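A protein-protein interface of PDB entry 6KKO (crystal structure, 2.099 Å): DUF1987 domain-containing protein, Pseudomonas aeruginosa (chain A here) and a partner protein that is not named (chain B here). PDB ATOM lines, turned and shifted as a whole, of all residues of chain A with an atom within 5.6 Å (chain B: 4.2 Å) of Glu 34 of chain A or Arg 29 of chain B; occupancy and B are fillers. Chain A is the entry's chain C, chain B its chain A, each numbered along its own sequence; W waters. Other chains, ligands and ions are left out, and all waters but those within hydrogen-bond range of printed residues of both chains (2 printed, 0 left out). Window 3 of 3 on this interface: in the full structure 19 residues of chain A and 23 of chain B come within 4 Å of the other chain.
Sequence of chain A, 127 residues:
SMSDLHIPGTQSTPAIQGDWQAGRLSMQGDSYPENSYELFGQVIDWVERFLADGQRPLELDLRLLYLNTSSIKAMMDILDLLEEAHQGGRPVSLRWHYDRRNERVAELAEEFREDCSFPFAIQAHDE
NH1 of Arg 29 of chain B lies within hydrogen-bond range of OG of Ser 12 of chain A (3.3 Å).
The side-chain hydroxyl (OG) of Ser 12 of chain A lies within hydrogen-bond range of the side-chain carboxylate (OE1) of Glu 33 of chain B (2.9 Å).
The side-chain carboxylate (OE2) of Glu 34 of chain A lies within salt-bridge range of the guanidinium group (NE) of Arg 68 of chain B, 2.5 Å away.
N of Glu 34 of chain A sits close to NH2 of Arg 29 of chain B, at 2.9 Å.
Glu 34 of chain A touches just these residues of chain B: Arg 29 (2.9 Å), Arg 68 (2.5 Å) and His 69 (3.6 Å).
Of the printed residues of chain A, Arg 29 of chain B touches Ser 12 (3.3 Å), Pro 33 (3.4 Å) and Glu 34 (2.9 Å).
Of the printed residues of chain A, His 69 of chain B touches Glu 34 (3.6 Å).
Printed residues of chain B within 4 Å of Pro 33 of chain A: Arg 29.
Printed residues of chain A within 4 Å of Arg 68 of chain B: Glu 34 (2.5 Å).
Printed residues of chain A within 4 Å of Glu 33 of chain B: Ser 12.
Ile 32 of chain B touches none of the printed residues of chain A.
Ser 70 of chain A touches none of the printed residues of chain B.
The nearest printed residue of chain B that does not touch Pro 33 of chain A is Glu 33 of chain B (5.8 Å).
Among the printed residues, merely in contact across the chains: Pro 33 of chain A with Arg 29 of chain B (3.4 Å) and Glu 34 of chain A with His 69 of chain B (3.6 Å).
Of the 8 printed residues of chain B, 4 touch a printed residue of chain A.
Hydrophobic or aromatic side chains of chain B that line the printed part of chain A: His 69.
Water W1 bridges O of Glu 33 of chain B (2.9 Å) and OH of Tyr 32 of chain A (2.9 Å).
Water W2 lies within hydrogen-bond range of the backbone carbonyl oxygen of Tyr 32 of chain A (2.9 Å), the side-chain carboxylate of Glu 33 of chain B (3.1 Å) and the guanidinium group of Arg 29 of chain B (3.4 Å).
The guanidinium group (NE) of Arg 29 of chain B is in salt-bridge range of the side-chain carboxylate (OE1) of Glu 33 of chain B, at 3.6 Å.
O of Ser 12 of chain A sits at hydrogen-bond distance from N of Tyr 32 of chain A (2.7 Å).
The backbone carbonyl oxygen (O) of Pro 33 of chain A is in hydrogen-bond range of the side-chain amide nitrogen (ND2) of Asn 68 of chain A (3.0 Å).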
ATOM      1  N   SER A  12      21.475 -22.549 -27.546  1.00  0.00           N
ATOM      2  CA  SER A  12      21.189 -21.418 -26.675  1.00  0.00           C
ATOM      3  C   SER A  12      21.909 -21.463 -25.334  1.00  0.00           C
ATOM      4  O   SER A  12      21.670 -20.586 -24.497  1.00  0.00           O
ATOM      5  CB  SER A  12      19.681 -21.312 -26.430  1.00  0.00           C
ATOM      6  OG  SER A  12      19.224 -22.439 -25.711  1.00  0.00           O
ATOM      7  N   THR A  13      22.754 -22.466 -25.089  1.00  0.00           N
ATOM      8  CA  THR A  13      23.489 -22.577 -23.840  1.00  0.00           C
ATOM      9  C   THR A  13      24.945 -22.914 -24.127  1.00  0.00           C
ATOM     10  O   THR A  13      25.235 -23.697 -25.037  1.00  0.00           O
ATOM     11  CB  THR A  13      22.902 -23.659 -22.919  1.00  0.00           C
ATOM     12  OG1 THR A  13      22.968 -24.931 -23.579  1.00  0.00           O
ATOM     13  CG2 THR A  13      21.461 -23.335 -22.530  1.00  0.00           C
ATOM     14  N   TYR A  32      21.666 -17.947 -24.011  1.00  0.00           N
ATOM     15  CA  TYR A  32      20.411 -17.235 -23.796  1.00  0.00           C
ATOM     16  C   TYR A  32      19.268 -18.171 -23.421  1.00  0.00           C
ATOM     17  O   TYR A  32      18.187 -18.098 -24.017  1.00  0.00           O
ATOM     18  CB  TYR A  32      20.049 -16.399 -25.029  1.00  0.00           C
ATOM     19  CG  TYR A  32      20.046 -17.131 -26.356  1.00  0.00           C
ATOM     20  CD1 TYR A  32      21.230 -17.376 -27.035  1.00  0.00           C
ATOM     21  CD2 TYR A  32      18.852 -17.523 -26.960  1.00  0.00           C
ATOM     22  CE1 TYR A  32      21.239 -18.025 -28.260  1.00  0.00           C
ATOM     23  CE2 TYR A  32      18.851 -18.163 -28.187  1.00  0.00           C
ATOM     24  CZ  TYR A  32      20.045 -18.415 -28.828  1.00  0.00           C
ATOM     25  OH  TYR A  32      20.076 -19.048 -30.049  1.00  0.00           O
ATOM     26  N   PRO A  33      19.431 -19.010 -22.400  1.00  0.00           N
ATOM     27  CA  PRO A  33      18.300 -19.809 -21.940  1.00  0.00           C
ATOM     28  C   PRO A  33      17.299 -18.942 -21.195  1.00  0.00           C
ATOM     29  O   PRO A  33      17.606 -17.845 -20.722  1.00  0.00           O
ATOM     30  CB  PRO A  33      18.950 -20.833 -21.007  1.00  0.00           C
ATOM     31  CG  PRO A  33      20.075 -20.084 -20.402  1.00  0.00           C
ATOM     32  CD  PRO A  33      20.563 -19.097 -21.455  1.00  0.00           C
ATOM     33  N   GLU A  34      16.075 -19.462 -21.100  1.00  0.00           N
ATOM     34  CA  GLU A  34      14.996 -18.734 -20.444  1.00  0.00           C
ATOM     35  C   GLU A  34      15.224 -18.652 -18.943  1.00  0.00           C
ATOM     36  O   GLU A  34      14.960 -17.616 -18.326  1.00  0.00           O
ATOM     37  CB  GLU A  34      13.653 -19.408 -20.725  1.00  0.00           C
ATOM     38  CG  GLU A  34      13.183 -19.393 -22.165  1.00  0.00           C
ATOM     39  CD  GLU A  34      11.679 -19.600 -22.273  1.00  0.00           C
ATOM     40  OE1 GLU A  34      11.123 -20.386 -21.472  1.00  0.00           O
ATOM     41  OE2 GLU A  34      11.054 -18.969 -23.151  1.00  0.00           O
ATOM     42  N   ASN A  35      15.698 -19.732 -18.337  1.00  0.00           N
ATOM     43  CA  ASN A  35      16.025 -19.758 -16.916  1.00  0.00           C
ATOM     44  C   ASN A  35      17.498 -20.131 -16.814  1.00  0.00           C
ATOM     45  O   ASN A  35      17.852 -21.313 -16.857  1.00  0.00           O
ATOM     46  CB  ASN A  35      15.124 -20.733 -16.161  1.00  0.00           C
ATOM     47  CG  ASN A  35      15.321 -20.675 -14.653  1.00  0.00           C
ATOM     48  OD1 ASN A  35      16.140 -19.908 -14.146  1.00  0.00           O
ATOM     49  ND2 ASN A  35      14.543 -21.474 -13.926  1.00  0.00           N
ATOM     50  N   SER A  36      18.358 -19.118 -16.697  1.00  0.00           N
ATOM     51  CA  SER A  36      19.791 -19.374 -16.708  1.00  0.00           C
ATOM     52  C   SER A  36      20.255 -20.090 -15.450  1.00  0.00           C
ATOM     53  O   SER A  36      21.327 -20.702 -15.463  1.00  0.00           O
ATOM     54  CB  SER A  36      20.558 -18.059 -16.885  1.00  0.00           C
ATOM     55  OG  SER A  36      20.364 -17.203 -15.769  1.00  0.00           O
ATOM     56  N   ASN A  68      22.293 -13.268 -22.674  1.00  0.00           N
ATOM     57  CA  ASN A  68      21.067 -12.525 -22.397  1.00  0.00           C
ATOM     58  C   ASN A  68      21.126 -11.996 -20.959  1.00  0.00           C
ATOM     59  O   ASN A  68      22.109 -12.230 -20.261  1.00  0.00           O
ATOM     60  CB  ASN A  68      19.818 -13.404 -22.644  1.00  0.00           C
ATOM     61  CG  ASN A  68      19.685 -14.560 -21.651  1.00  0.00           C
ATOM     62  OD1 ASN A  68      20.624 -14.919 -20.944  1.00  0.00           O
ATOM     63  ND2 ASN A  68      18.496 -15.161 -21.617  1.00  0.00           N
ATOM     64  N   SER A  70      19.522 -12.676 -18.161  1.00  0.00           N
ATOM     65  CA  SER A  70      19.561 -13.684 -17.104  1.00  0.00           C
ATOM     66  C   SER A  70      20.954 -14.291 -16.960  1.00  0.00           C
ATOM     67  O   SER A  70      21.435 -14.490 -15.851  1.00  0.00           O
ATOM     68  CB  SER A  70      18.543 -14.793 -17.383  1.00  0.00           C
ATOM     69  OG  SER A  70      18.520 -15.733 -16.326  1.00  0.00           O
ATOM     70  N   SER B  28       6.781 -20.084 -28.281  1.00  0.00           N
ATOM     71  CA  SER B  28       7.432 -20.987 -27.352  1.00  0.00           C
ATOM     72  C   SER B  28       8.931 -20.729 -27.333  1.00  0.00           C
ATOM     73  O   SER B  28       9.491 -20.073 -28.216  1.00  0.00           O
ATOM     74  CB  SER B  28       7.171 -22.441 -27.737  1.00  0.00           C
ATOM     75  OG  SER B  28       7.878 -22.773 -28.918  1.00  0.00           O
ATOM     76  N   ARG B  29       9.590 -21.336 -26.366  1.00  0.00           N
ATOM     77  CA  ARG B  29      11.040 -21.264 -26.244  1.00  0.00           C
ATOM     78  C   ARG B  29      11.688 -21.679 -27.522  1.00  0.00           C
ATOM     79  O   ARG B  29      12.474 -20.956 -28.058  1.00  0.00           O
ATOM     80  CB  ARG B  29      11.583 -22.151 -25.148  1.00  0.00           C
ATOM     81  CG  ARG B  29      13.075 -22.111 -25.036  1.00  0.00           C
ATOM     82  CD  ARG B  29      13.578 -22.949 -23.879  1.00  0.00           C
ATOM     83  NE  ARG B  29      14.982 -23.397 -23.969  1.00  0.00           N
ATOM     84  CZ  ARG B  29      15.974 -22.959 -23.185  1.00  0.00           C
ATOM     85  NH1 ARG B  29      17.228 -23.402 -23.333  1.00  0.00           N
ATOM     86  NH2 ARG B  29      15.727 -22.069 -22.259  1.00  0.00           N
ATOM     87  N   SER B  30      11.326 -22.856 -27.999  1.00  0.00           N
ATOM     88  CA  SER B  30      11.929 -23.383 -29.219  1.00  0.00           C
ATOM     89  C   SER B  30      11.543 -22.556 -30.438  1.00  0.00           C
ATOM     90  O   SER B  30      12.331 -22.439 -31.384  1.00  0.00           O
ATOM     91  CB  SER B  30      11.520 -24.839 -29.420  1.00  0.00           C
ATOM     92  OG  SER B  30      11.819 -25.606 -28.264  1.00  0.00           O
ATOM     93  N   LEU B  31      10.352 -21.952 -30.429  1.00  0.00           N
ATOM     94  CA  LEU B  31       9.971 -21.105 -31.550  1.00  0.00           C
ATOM     95  C   LEU B  31      10.798 -19.819 -31.551  1.00  0.00           C
ATOM     96  O   LEU B  31      11.224 -19.348 -32.616  1.00  0.00           O
ATOM     97  CB  LEU B  31       8.468 -20.833 -31.479  1.00  0.00           C
ATOM     98  CG  LEU B  31       7.634 -20.569 -32.736  1.00  0.00           C
ATOM     99  CD1 LEU B  31       6.150 -20.687 -32.410  1.00  0.00           C
ATOM    100  CD2 LEU B  31       7.920 -19.226 -33.310  1.00  0.00           C
ATOM    101  N   ILE B  32      11.083 -19.272 -30.360  1.00  0.00           N
ATOM    102  CA  ILE B  32      11.965 -18.105 -30.240  1.00  0.00           C
ATOM    103  C   ILE B  32      13.309 -18.379 -30.893  1.00  0.00           C
ATOM    104  O   ILE B  32      13.813 -17.575 -31.688  1.00  0.00           O
ATOM    105  CB  ILE B  32      12.162 -17.723 -28.764  1.00  0.00           C
ATOM    106  CG1 ILE B  32      10.842 -17.342 -28.123  1.00  0.00           C
ATOM    107  CG2 ILE B  32      13.178 -16.590 -28.644  1.00  0.00           C
ATOM    108  CD1 ILE B  32      10.504 -15.963 -28.369  1.00  0.00           C
ATOM    109  N   GLU B  33      13.916 -19.520 -30.552  1.00  0.00           N
ATOM    110  CA  GLU B  33      15.254 -19.826 -31.035  1.00  0.00           C
ATOM    111  C   GLU B  33      15.257 -20.053 -32.535  1.00  0.00           C
ATOM    112  O   GLU B  33      16.189 -19.632 -33.232  1.00  0.00           O
ATOM    113  CB  GLU B  33      15.798 -21.063 -30.326  1.00  0.00           C
ATOM    114  CG  GLU B  33      15.900 -20.946 -28.821  1.00  0.00           C
ATOM    115  CD  GLU B  33      16.616 -22.131 -28.213  1.00  0.00           C
ATOM    116  OE1 GLU B  33      16.610 -22.254 -26.971  1.00  0.00           O
ATOM    117  OE2 GLU B  33      17.172 -22.946 -28.984  1.00  0.00           O
ATOM    118  N   ARG B  68       7.817 -13.877 -22.797  1.00  0.00           N
ATOM    119  CA  ARG B  68       7.766 -15.164 -22.114  1.00  0.00           C
ATOM    120  C   ARG B  68       7.733 -14.989 -20.605  1.00  0.00           C
ATOM    121  O   ARG B  68       6.941 -15.644 -19.918  1.00  0.00           O
ATOM    122  CB  ARG B  68       8.960 -16.018 -22.521  1.00  0.00           C
ATOM    123  CG  ARG B  68       8.974 -16.373 -23.988  1.00  0.00           C
ATOM    124  CD  ARG B  68       8.081 -17.557 -24.221  1.00  0.00           C
ATOM    125  NE  ARG B  68       8.540 -18.690 -23.427  1.00  0.00           N
ATOM    126  CZ  ARG B  68       7.812 -19.774 -23.194  1.00  0.00           C
ATOM    127  NH1 ARG B  68       6.588 -19.871 -23.697  1.00  0.00           N
ATOM    128  NH2 ARG B  68       8.311 -20.760 -22.461  1.00  0.00           N
ATOM    129  N   HIS B  69       8.581 -14.103 -20.069  1.00  0.00           N
ATOM    130  CA  HIS B  69       8.647 -13.909 -18.623  1.00  0.00           C
ATOM    131  C   HIS B  69       7.338 -13.356 -18.085  1.00  0.00           C
ATOM    132  O   HIS B  69       6.882 -13.756 -17.006  1.00  0.00           O
ATOM    133  CB  HIS B  69       9.805 -12.975 -18.261  1.00  0.00           C
ATOM    134  CG  HIS B  69      11.157 -13.515 -18.616  1.00  0.00           C
ATOM    135  ND1 HIS B  69      12.255 -12.703 -18.811  1.00  0.00           N
ATOM    136  CD2 HIS B  69      11.588 -14.784 -18.813  1.00  0.00           C
ATOM    137  CE1 HIS B  69      13.302 -13.448 -19.113  1.00  0.00           C
ATOM    138  NE2 HIS B  69      12.926 -14.714 -19.122  1.00  0.00           N
HETATM  139  O   HOH W   1      18.690 -18.423 -32.515  1.00  0.00           O
HETATM  140  O   HOH W   2      16.179 -20.003 -24.898  1.00  0.00           O
